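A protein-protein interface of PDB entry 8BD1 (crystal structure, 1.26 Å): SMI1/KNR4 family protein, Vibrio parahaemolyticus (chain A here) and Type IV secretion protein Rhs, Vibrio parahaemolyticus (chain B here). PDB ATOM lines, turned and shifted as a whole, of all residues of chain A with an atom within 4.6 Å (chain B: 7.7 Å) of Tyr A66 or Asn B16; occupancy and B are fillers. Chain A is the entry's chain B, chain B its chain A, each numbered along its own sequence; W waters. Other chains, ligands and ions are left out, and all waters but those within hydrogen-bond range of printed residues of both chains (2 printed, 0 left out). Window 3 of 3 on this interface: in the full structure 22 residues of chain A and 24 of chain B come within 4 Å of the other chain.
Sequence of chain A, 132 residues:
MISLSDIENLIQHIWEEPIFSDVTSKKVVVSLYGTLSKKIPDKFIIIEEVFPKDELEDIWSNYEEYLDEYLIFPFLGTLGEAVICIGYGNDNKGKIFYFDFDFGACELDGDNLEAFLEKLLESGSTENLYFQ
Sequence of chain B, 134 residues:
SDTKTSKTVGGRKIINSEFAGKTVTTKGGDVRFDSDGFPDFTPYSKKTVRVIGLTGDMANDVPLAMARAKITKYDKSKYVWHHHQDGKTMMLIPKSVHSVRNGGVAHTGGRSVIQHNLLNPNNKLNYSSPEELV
Hydrophobic or aromatic side chains of chain A that line the printed part of chain B: Tyr A63, Tyr A66 and Phe A101. Along chain A the printed residues that touch a printed residue of chain B span positions 62 to 101. Along chain B the printed residues that touch a printed residue of chain A span positions 15 to 108.
CG1 of Val B100 touches CD2 of Tyr A63 (3.7 Å). Ala B106 touches Tyr A66 (CB to CZ, 3.4 Å). Phe A101 touches Ile B15 (O to CG1, 3.5 Å). Val B100 touches Phe A101 (CG2 to CE2, 3.7 Å). Phe A101 touches Ala B106 (CZ to CB, 3.6 Å). His B107 touches Phe A101.
Of chain A, only Tyr A66 (3.0 Å) comes within 4 Å of Asn B16. Of the printed residues of chain B, Asn A62 touches Val B100. Printed residues of chain A within 4 Å of Ala B106: Tyr A66 and Phe A101. Of the printed residues of chain B, Phe A101 touches Ile B15 (3.5 Å), Val B100 (3.7 Å), Ala B106 (3.6 Å), His B107 (3.2 Å) and Thr B108 (3.4 Å). Of the printed residues of chain A, Ile B15 touches Phe A101. Glu B18 touches none of the printed residues of chain A. The nearest residue of chain B that does not touch Tyr A66 is Val B100 (4.3 Å).
OG1 of Thr B108 sits at hydrogen-bond distance from N of Ile B15 (2.9 Å). ND2 of Asn B16 lies within hydrogen-bond range of O of Ala B106, at 2.9 Å. The backbone carbonyl oxygen (O) of Val B105 sits at hydrogen-bond distance from a ring nitrogen (ND1) of His B107 (2.9 Å).
OH of Tyr A66 sits at hydrogen-bond distance from ND2 of Asn B16, 3.0 Å away. The backbone carbonyl oxygen (O) of Val B100 sits at hydrogen-bond distance from the side-chain amide nitrogen (ND2) of Asn A62 (3.5 Å). The side-chain hydroxyl of Thr B108 is in hydrogen-bond range of the backbone carbonyl oxygen of Phe A101 (3.4 Å).
Water W1 bridges the side-chain hydroxyl of Tyr A66 (2.7 Å) and the backbone NH of Ala B106 (3.1 Å). Water W2 lies within hydrogen-bond range of OG1 of Thr B108, O of Lys B13 and O of Phe A101.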
ATOM      1  N   ASN A  62     -30.458   7.926  16.572  1.00  0.00           N
ATOM      2  CA  ASN A  62     -29.626   7.522  17.698  1.00  0.00           C
ATOM      3  C   ASN A  62     -29.500   6.010  17.838  1.00  0.00           C
ATOM      4  O   ASN A  62     -28.452   5.525  18.277  1.00  0.00           O
ATOM      5  CB  ASN A  62     -30.172   8.113  18.999  1.00  0.00           C
ATOM      6  CG  ASN A  62     -29.946   9.602  19.090  1.00  0.00           C
ATOM      7  OD1 ASN A  62     -28.950  10.112  18.574  1.00  0.00           O
ATOM      8  ND2 ASN A  62     -30.851  10.303  19.756  1.00  0.00           N
ATOM      9  N   TYR A  63     -30.527   5.258  17.461  1.00  0.00           N
ATOM     10  CA  TYR A  63     -30.522   3.815  17.652  1.00  0.00           C
ATOM     11  C   TYR A  63     -30.032   3.029  16.442  1.00  0.00           C
ATOM     12  O   TYR A  63     -29.681   1.852  16.597  1.00  0.00           O
ATOM     13  CB  TYR A  63     -31.932   3.320  17.993  1.00  0.00           C
ATOM     14  CG  TYR A  63     -32.093   3.034  19.464  1.00  0.00           C
ATOM     15  CD1 TYR A  63     -31.420   1.973  20.038  1.00  0.00           C
ATOM     16  CD2 TYR A  63     -32.914   3.815  20.280  1.00  0.00           C
ATOM     17  CE1 TYR A  63     -31.533   1.684  21.379  1.00  0.00           C
ATOM     18  CE2 TYR A  63     -33.037   3.524  21.642  1.00  0.00           C
ATOM     19  CZ  TYR A  63     -32.336   2.460  22.169  1.00  0.00           C
ATOM     20  OH  TYR A  63     -32.422   2.138  23.505  1.00  0.00           O
ATOM     21  N   GLU A  64     -30.020   3.643  15.248  1.00  0.00           N
ATOM     22  CA  GLU A  64     -29.780   2.898  14.011  1.00  0.00           C
ATOM     23  C   GLU A  64     -28.480   2.105  14.065  1.00  0.00           C
ATOM     24  O   GLU A  64     -28.446   0.935  13.664  1.00  0.00           O
ATOM     25  CB  GLU A  64     -29.771   3.855  12.821  1.00  0.00           C
ATOM     26  CG  GLU A  64     -29.559   3.184  11.475  1.00  0.00           C
ATOM     27  CD  GLU A  64     -29.736   4.154  10.325  1.00  0.00           C
ATOM     28  OE1 GLU A  64     -29.270   5.307  10.453  1.00  0.00           O
ATOM     29  OE2 GLU A  64     -30.341   3.771   9.300  1.00  0.00           O
ATOM     30  N   GLU A  65     -27.403   2.714  14.564  1.00  0.00           N
ATOM     31  CA  GLU A  65     -26.115   2.028  14.578  1.00  0.00           C
ATOM     32  C   GLU A  65     -26.138   0.780  15.453  1.00  0.00           C
ATOM     33  O   GLU A  65     -25.338  -0.137  15.236  1.00  0.00           O
ATOM     34  CB  GLU A  65     -25.008   2.982  15.033  1.00  0.00           C
ATOM     35  CG  GLU A  65     -25.048   3.312  16.517  1.00  0.00           C
ATOM     36  CD  GLU A  65     -23.979   4.301  16.935  1.00  0.00           C
ATOM     37  OE1 GLU A  65     -22.846   3.866  17.223  1.00  0.00           O
ATOM     38  OE2 GLU A  65     -24.281   5.513  16.988  1.00  0.00           O
ATOM     39  N   TYR A  66     -27.052   0.717  16.421  1.00  0.00           N
ATOM     40  CA  TYR A  66     -27.130  -0.419  17.327  1.00  0.00           C
ATOM     41  C   TYR A  66     -28.121  -1.481  16.879  1.00  0.00           C
ATOM     42  O   TYR A  66     -27.962  -2.653  17.245  1.00  0.00           O
ATOM     43  CB  TYR A  66     -27.498   0.074  18.730  1.00  0.00           C
ATOM     44  CG  TYR A  66     -26.530   1.105  19.239  1.00  0.00           C
ATOM     45  CD1 TYR A  66     -25.216   0.753  19.518  1.00  0.00           C
ATOM     46  CD2 TYR A  66     -26.915   2.425  19.423  1.00  0.00           C
ATOM     47  CE1 TYR A  66     -24.316   1.675  19.976  1.00  0.00           C
ATOM     48  CE2 TYR A  66     -26.016   3.364  19.885  1.00  0.00           C
ATOM     49  CZ  TYR A  66     -24.713   2.985  20.157  1.00  0.00           C
ATOM     50  OH  TYR A  66     -23.797   3.906  20.616  1.00  0.00           O
ATOM     51  N   LEU A  67     -29.147  -1.112  16.109  1.00  0.00           N
ATOM     52  CA  LEU A  67     -30.258  -2.010  15.838  1.00  0.00           C
ATOM     53  C   LEU A  67     -30.454  -2.373  14.375  1.00  0.00           C
ATOM     54  O   LEU A  67     -31.245  -3.281  14.095  1.00  0.00           O
ATOM     55  CB  LEU A  67     -31.572  -1.418  16.375  1.00  0.00           C
ATOM     56  CG  LEU A  67     -31.633  -1.329  17.897  1.00  0.00           C
ATOM     57  CD1 LEU A  67     -32.959  -0.717  18.315  1.00  0.00           C
ATOM     58  CD2 LEU A  67     -31.472  -2.701  18.511  1.00  0.00           C
ATOM     59  N   ASP A  68     -29.778  -1.700  13.437  1.00  0.00           N
ATOM     60  CA  ASP A  68     -30.099  -1.942  12.032  1.00  0.00           C
ATOM     61  C   ASP A  68     -29.752  -3.362  11.596  1.00  0.00           C
ATOM     62  O   ASP A  68     -30.386  -3.894  10.684  1.00  0.00           O
ATOM     63  CB  ASP A  68     -29.509  -0.873  11.097  1.00  0.00           C
ATOM     64  CG  ASP A  68     -28.008  -0.697  11.244  1.00  0.00           C
ATOM     65  OD1 ASP A  68     -27.351  -1.509  11.925  1.00  0.00           O
ATOM     66  OD2 ASP A  68     -27.476   0.272  10.657  1.00  0.00           O
ATOM     67  N   TYR A  70     -30.153  -6.098  13.439  1.00  0.00           N
ATOM     68  CA  TYR A  70     -31.228  -6.958  13.905  1.00  0.00           C
ATOM     69  C   TYR A  70     -32.517  -6.734  13.129  1.00  0.00           C
ATOM     70  O   TYR A  70     -33.428  -7.562  13.223  1.00  0.00           O
ATOM     71  CB  TYR A  70     -31.530  -6.685  15.382  1.00  0.00           C
ATOM     72  CG  TYR A  70     -30.366  -6.881  16.332  1.00  0.00           C
ATOM     73  CD1 TYR A  70     -29.991  -8.145  16.767  1.00  0.00           C
ATOM     74  CD2 TYR A  70     -29.665  -5.792  16.817  1.00  0.00           C
ATOM     75  CE1 TYR A  70     -28.929  -8.309  17.657  1.00  0.00           C
ATOM     76  CE2 TYR A  70     -28.607  -5.949  17.698  1.00  0.00           C
ATOM     77  CZ  TYR A  70     -28.251  -7.209  18.109  1.00  0.00           C
ATOM     78  OH  TYR A  70     -27.198  -7.347  18.993  1.00  0.00           O
ATOM     79  N   PHE A 101     -28.805  -3.420  26.119  1.00  0.00           N
ATOM     80  CA  PHE A 101     -27.372  -3.367  25.871  1.00  0.00           C
ATOM     81  C   PHE A 101     -26.559  -4.246  26.808  1.00  0.00           C
ATOM     82  O   PHE A 101     -25.325  -4.278  26.692  1.00  0.00           O
ATOM     83  CB  PHE A 101     -26.880  -1.916  25.933  1.00  0.00           C
ATOM     84  CG  PHE A 101     -27.280  -1.092  24.743  1.00  0.00           C
ATOM     85  CD1 PHE A 101     -26.795  -1.401  23.484  1.00  0.00           C
ATOM     86  CD2 PHE A 101     -28.143  -0.019  24.875  1.00  0.00           C
ATOM     87  CE1 PHE A 101     -27.164  -0.658  22.378  1.00  0.00           C
ATOM     88  CE2 PHE A 101     -28.509   0.730  23.772  1.00  0.00           C
ATOM     89  CZ  PHE A 101     -28.017   0.407  22.524  1.00  0.00           C
ATOM     90  N   LYS B   7     -12.556  -6.771  26.793  1.00  0.00           N
ATOM     91  CA  LYS B   7     -13.645  -5.971  27.344  1.00  0.00           C
ATOM     92  C   LYS B   7     -15.001  -6.620  27.069  1.00  0.00           C
ATOM     93  O   LYS B   7     -15.761  -6.179  26.199  1.00  0.00           O
ATOM     94  CB  LYS B   7     -13.602  -4.546  26.792  1.00  0.00           C
ATOM     95  N   LYS B  13     -19.420  -8.387  24.034  1.00  0.00           N
ATOM     96  CA  LYS B  13     -18.630  -7.167  24.000  1.00  0.00           C
ATOM     97  C   LYS B  13     -19.302  -6.076  24.826  1.00  0.00           C
ATOM     98  O   LYS B  13     -20.509  -5.842  24.705  1.00  0.00           O
ATOM     99  CB  LYS B  13     -18.492  -6.688  22.557  1.00  0.00           C
ATOM    100  CG  LYS B  13     -17.614  -5.458  22.407  1.00  0.00           C
ATOM    101  CD  LYS B  13     -17.981  -4.640  21.174  1.00  0.00           C
ATOM    102  CE  LYS B  13     -17.589  -3.177  21.366  1.00  0.00           C
ATOM    103  NZ  LYS B  13     -17.768  -2.357  20.134  1.00  0.00           N
ATOM    104  N   ILE B  14     -18.519  -5.406  25.671  1.00  0.00           N
ATOM    105  CA  ILE B  14     -19.031  -4.239  26.383  1.00  0.00           C
ATOM    106  C   ILE B  14     -19.357  -3.153  25.371  1.00  0.00           C
ATOM    107  O   ILE B  14     -18.521  -2.781  24.540  1.00  0.00           O
ATOM    108  CB  ILE B  14     -18.013  -3.767  27.436  1.00  0.00           C
ATOM    109  CG1 ILE B  14     -17.969  -4.738  28.617  1.00  0.00           C
ATOM    110  CG2 ILE B  14     -18.333  -2.345  27.916  1.00  0.00           C
ATOM    111  CD1 ILE B  14     -16.828  -4.462  29.591  1.00  0.00           C
ATOM    112  N   ILE B  15     -20.590  -2.645  25.420  1.00  0.00           N
ATOM    113  CA  ILE B  15     -21.056  -1.708  24.406  1.00  0.00           C
ATOM    114  C   ILE B  15     -20.256  -0.414  24.498  1.00  0.00           C
ATOM    115  O   ILE B  15     -20.071   0.151  25.585  1.00  0.00           O
ATOM    116  CB  ILE B  15     -22.563  -1.469  24.570  1.00  0.00           C
ATOM    117  CG1 ILE B  15     -23.345  -2.757  24.289  1.00  0.00           C
ATOM    118  CG2 ILE B  15     -23.019  -0.325  23.663  1.00  0.00           C
ATOM    119  CD1 ILE B  15     -23.330  -3.184  22.824  1.00  0.00           C
ATOM    120  N   ASN B  16     -19.755   0.046  23.348  1.00  0.00           N
ATOM    121  CA  ASN B  16     -18.919   1.246  23.254  1.00  0.00           C
ATOM    122  C   ASN B  16     -17.623   1.130  24.055  1.00  0.00           C
ATOM    123  O   ASN B  16     -17.041   2.137  24.465  1.00  0.00           O
ATOM    124  CB  ASN B  16     -19.691   2.524  23.594  1.00  0.00           C
ATOM    125  CG  ASN B  16     -20.587   2.965  22.464  1.00  0.00           C
ATOM    126  OD1 ASN B  16     -20.222   2.856  21.293  1.00  0.00           O
ATOM    127  ND2 ASN B  16     -21.778   3.447  22.803  1.00  0.00           N
ATOM    128  N   SER B  17     -17.150  -0.101  24.277  1.00  0.00           N
ATOM    129  CA  SER B  17     -15.895  -0.285  24.998  1.00  0.00           C
ATOM    130  C   SER B  17     -14.701   0.249  24.223  1.00  0.00           C
ATOM    131  O   SER B  17     -13.644   0.478  24.819  1.00  0.00           O
ATOM    132  CB  SER B  17     -15.684  -1.756  25.368  1.00  0.00           C
ATOM    133  OG  SER B  17     -15.807  -2.595  24.238  1.00  0.00           O
ATOM    134  N   GLU B  18     -14.855   0.468  22.916  1.00  0.00           N
ATOM    135  CA  GLU B  18     -13.802   1.089  22.123  1.00  0.00           C
ATOM    136  C   GLU B  18     -13.521   2.526  22.546  1.00  0.00           C
ATOM    137  O   GLU B  18     -12.551   3.117  22.057  1.00  0.00           O
ATOM    138  CB  GLU B  18     -14.159   1.013  20.633  1.00  0.00           C
ATOM    139  CG  GLU B  18     -15.402   1.798  20.228  1.00  0.00           C
ATOM    140  CD  GLU B  18     -16.645   0.924  20.069  1.00  0.00           C
ATOM    141  OE1 GLU B  18     -16.829  -0.029  20.864  1.00  0.00           O
ATOM    142  OE2 GLU B  18     -17.434   1.190  19.136  1.00  0.00           O
ATOM    143  N   PHE B  19     -14.331   3.097  23.436  1.00  0.00           N
ATOM    144  CA  PHE B  19     -14.084   4.415  24.006  1.00  0.00           C
ATOM    145  C   PHE B  19     -13.507   4.350  25.416  1.00  0.00           C
ATOM    146  O   PHE B  19     -13.517   5.362  26.123  1.00  0.00           O
ATOM    147  CB  PHE B  19     -15.368   5.249  23.998  1.00  0.00           C
ATOM    148  CG  PHE B  19     -15.897   5.540  22.620  1.00  0.00           C
ATOM    149  CD1 PHE B  19     -15.213   6.386  21.762  1.00  0.00           C
ATOM    150  CD2 PHE B  19     -17.077   4.961  22.183  1.00  0.00           C
ATOM    151  CE1 PHE B  19     -15.701   6.653  20.493  1.00  0.00           C
ATOM    152  CE2 PHE B  19     -17.570   5.224  20.918  1.00  0.00           C
ATOM    153  CZ  PHE B  19     -16.882   6.071  20.072  1.00  0.00           C
ATOM    154  N   ALA B  20     -13.008   3.189  25.843  1.00  0.00           N
ATOM    155  CA  ALA B  20     -12.406   3.066  27.164  1.00  0.00           C
ATOM    156  C   ALA B  20     -11.252   4.049  27.316  1.00  0.00           C
ATOM    157  O   ALA B  20     -10.414   4.185  26.419  1.00  0.00           O
ATOM    158  CB  ALA B  20     -11.903   1.638  27.376  1.00  0.00           C
ATOM    159  N   GLY B  21     -11.210   4.733  28.456  1.00  0.00           N
ATOM    160  CA  GLY B  21     -10.228   5.772  28.688  1.00  0.00           C
ATOM    161  C   GLY B  21     -10.455   7.054  27.918  1.00  0.00           C
ATOM    162  O   GLY B  21      -9.626   7.967  28.015  1.00  0.00           O
ATOM    163  N   VAL B  24     -16.791  10.877  25.757  1.00  0.00           N
ATOM    164  CA  VAL B  24     -17.764  11.009  24.682  1.00  0.00           C
ATOM    165  C   VAL B  24     -18.765  12.094  25.049  1.00  0.00           C
ATOM    166  O   VAL B  24     -19.035  12.353  26.227  1.00  0.00           O
ATOM    167  CB  VAL B  24     -18.469   9.675  24.347  1.00  0.00           C
ATOM    168  CG1 VAL B  24     -17.461   8.528  24.325  1.00  0.00           C
ATOM    169  CG2 VAL B  24     -19.571   9.390  25.348  1.00  0.00           C
ATOM    170  N   PHE B  33     -15.495   7.323  29.822  1.00  0.00           N
ATOM    171  CA  PHE B  33     -15.481   5.871  29.958  1.00  0.00           C
ATOM    172  C   PHE B  33     -14.174   5.454  30.623  1.00  0.00           C
ATOM    173  O   PHE B  33     -13.098   5.932  30.242  1.00  0.00           O
ATOM    174  CB  PHE B  33     -15.615   5.198  28.591  1.00  0.00           C
ATOM    175  CG  PHE B  33     -17.035   5.093  28.101  1.00  0.00           C
ATOM    176  CD1 PHE B  33     -17.759   6.228  27.784  1.00  0.00           C
ATOM    177  CD2 PHE B  33     -17.646   3.853  27.959  1.00  0.00           C
ATOM    178  CE1 PHE B  33     -19.068   6.139  27.333  1.00  0.00           C
ATOM    179  CE2 PHE B  33     -18.953   3.754  27.504  1.00  0.00           C
ATOM    180  CZ  PHE B  33     -19.666   4.903  27.193  1.00  0.00           C
ATOM    181  N   ASP B  34     -14.263   4.572  31.617  1.00  0.00           N
ATOM    182  CA  ASP B  34     -13.081   4.177  32.371  1.00  0.00           C
ATOM    183  C   ASP B  34     -12.259   3.134  31.609  1.00  0.00           C
ATOM    184  O   ASP B  34     -12.577   2.750  30.482  1.00  0.00           O
ATOM    185  CB  ASP B  34     -13.453   3.755  33.794  1.00  0.00           C
ATOM    186  CG  ASP B  34     -14.295   2.485  33.850  1.00  0.00           C
ATOM    187  OD1 ASP B  34     -14.221   1.633  32.936  1.00  0.00           O
ATOM    188  OD2 ASP B  34     -15.020   2.336  34.852  1.00  0.00           O
ATOM    189  N   ASP B  36     -12.014   0.029  31.910  1.00  0.00           N
ATOM    190  CA  ASP B  36     -12.690  -1.225  31.603  1.00  0.00           C
ATOM    191  C   ASP B  36     -13.778  -1.072  30.550  1.00  0.00           C
ATOM    192  O   ASP B  36     -14.361  -2.080  30.140  1.00  0.00           O
ATOM    193  CB  ASP B  36     -13.274  -1.833  32.873  1.00  0.00           C
ATOM    194  CG  ASP B  36     -12.227  -2.048  33.933  1.00  0.00           C
ATOM    195  OD1 ASP B  36     -11.317  -2.870  33.706  1.00  0.00           O
ATOM    196  OD2 ASP B  36     -12.317  -1.387  34.981  1.00  0.00           O
ATOM    197  N   GLY B  37     -14.041   0.143  30.087  1.00  0.00           N
ATOM    198  CA  GLY B  37     -15.096   0.376  29.124  1.00  0.00           C
ATOM    199  C   GLY B  37     -16.445   0.725  29.714  1.00  0.00           C
ATOM    200  O   GLY B  37     -17.448   0.660  28.995  1.00  0.00           O
ATOM    201  N   PHE B  38     -16.507   1.075  30.992  1.00  0.00           N
ATOM    202  CA  PHE B  38     -17.763   1.464  31.617  1.00  0.00           C
ATOM    203  C   PHE B  38     -17.837   2.978  31.765  1.00  0.00           C
ATOM    204  O   PHE B  38     -16.853   3.616  32.165  1.00  0.00           O
ATOM    205  CB  PHE B  38     -17.903   0.845  33.007  1.00  0.00           C
ATOM    206  CG  PHE B  38     -18.014  -0.651  32.994  1.00  0.00           C
ATOM    207  CD1 PHE B  38     -19.103  -1.279  32.401  1.00  0.00           C
ATOM    208  CD2 PHE B  38     -17.028  -1.437  33.567  1.00  0.00           C
ATOM    209  CE1 PHE B  38     -19.209  -2.659  32.385  1.00  0.00           C
ATOM    210  CE2 PHE B  38     -17.124  -2.822  33.554  1.00  0.00           C
ATOM    211  CZ  PHE B  38     -18.213  -3.436  32.957  1.00  0.00           C
ATOM    212  N   PRO B  39     -18.987   3.573  31.477  1.00  0.00           N
ATOM    213  CA  PRO B  39     -19.139   5.016  31.678  1.00  0.00           C
ATOM    214  C   PRO B  39     -19.070   5.360  33.153  1.00  0.00           C
ATOM    215  O   PRO B  39     -19.461   4.572  34.017  1.00  0.00           O
ATOM    216  CB  PRO B  39     -20.541   5.297  31.129  1.00  0.00           C
ATOM    217  CG  PRO B  39     -21.261   3.982  31.298  1.00  0.00           C
ATOM    218  CD  PRO B  39     -20.235   2.942  31.011  1.00  0.00           C
ATOM    219  N   VAL B 100     -30.036   6.135  25.183  1.00  0.00           N
ATOM    220  CA  VAL B 100     -29.898   6.388  23.747  1.00  0.00           C
ATOM    221  C   VAL B 100     -31.095   7.166  23.218  1.00  0.00           C
ATOM    222  O   VAL B 100     -30.948   8.087  22.405  1.00  0.00           O
ATOM    223  CB  VAL B 100     -29.697   5.060  22.988  1.00  0.00           C
ATOM    224  CG1 VAL B 100     -29.781   5.283  21.474  1.00  0.00           C
ATOM    225  CG2 VAL B 100     -28.376   4.443  23.362  1.00  0.00           C
ATOM    226  N   GLY B 104     -28.447  10.153  25.190  1.00  0.00           N
ATOM    227  CA  GLY B 104     -27.382   9.627  26.016  1.00  0.00           C
ATOM    228  C   GLY B 104     -26.546   8.620  25.256  1.00  0.00           C
ATOM    229  O   GLY B 104     -26.739   8.384  24.065  1.00  0.00           O
ATOM    230  N   VAL B 105     -25.610   7.991  25.965  1.00  0.00           N
ATOM    231  CA  VAL B 105     -24.637   7.095  25.347  1.00  0.00           C
ATOM    232  C   VAL B 105     -24.969   5.649  25.691  1.00  0.00           C
ATOM    233  O   VAL B 105     -25.161   5.311  26.865  1.00  0.00           O
ATOM    234  CB  VAL B 105     -23.186   7.459  25.719  1.00  0.00           C
ATOM    235  CG1 VAL B 105     -22.976   7.498  27.233  1.00  0.00           C
ATOM    236  CG2 VAL B 105     -22.204   6.498  25.041  1.00  0.00           C
ATOM    237  N   ALA B 106     -25.021   4.796  24.665  1.00  0.00           N
ATOM    238  CA  ALA B 106     -25.214   3.368  24.875  1.00  0.00           C
ATOM    239  C   ALA B 106     -24.042   2.786  25.653  1.00  0.00           C
ATOM    240  O   ALA B 106     -22.885   3.156  25.442  1.00  0.00           O
ATOM    241  CB  ALA B 106     -25.322   2.653  23.526  1.00  0.00           C
ATOM    242  N   HIS B 107     -24.338   1.850  26.545  1.00  0.00           N
ATOM    243  CA  HIS B 107     -23.298   1.290  27.393  1.00  0.00           C
ATOM    244  C   HIS B 107     -23.818   0.007  28.026  1.00  0.00           C
ATOM    245  O   HIS B 107     -25.016  -0.284  27.999  1.00  0.00           O
ATOM    246  CB  HIS B 107     -22.912   2.279  28.490  1.00  0.00           C
ATOM    247  CG  HIS B 107     -24.044   2.591  29.414  1.00  0.00           C
ATOM    248  ND1 HIS B 107     -24.999   3.544  29.129  1.00  0.00           N
ATOM    249  CD2 HIS B 107     -24.409   2.030  30.589  1.00  0.00           C
ATOM    250  CE1 HIS B 107     -25.897   3.560  30.099  1.00  0.00           C
ATOM    251  NE2 HIS B 107     -25.555   2.662  31.004  1.00  0.00           N
ATOM    252  N   THR B 108     -22.891  -0.743  28.605  1.00  0.00           N
ATOM    253  CA  THR B 108     -23.170  -1.928  29.399  1.00  0.00           C
ATOM    254  C   THR B 108     -23.051  -1.564  30.874  1.00  0.00           C
ATOM    255  O   THR B 108     -22.194  -0.760  31.253  1.00  0.00           O
ATOM    256  CB  THR B 108     -22.137  -3.001  29.045  1.00  0.00           C
ATOM    257  OG1 THR B 108     -22.246  -3.317  27.651  1.00  0.00           O
ATOM    258  CG2 THR B 108     -22.321  -4.261  29.868  1.00  0.00           C
HETATM  259  O   HOH W   1     -24.826   6.067  21.879  1.00  0.00           O
HETATM  260  O   HOH W   2     -22.566  -5.945  26.698  1.00  0.00           O
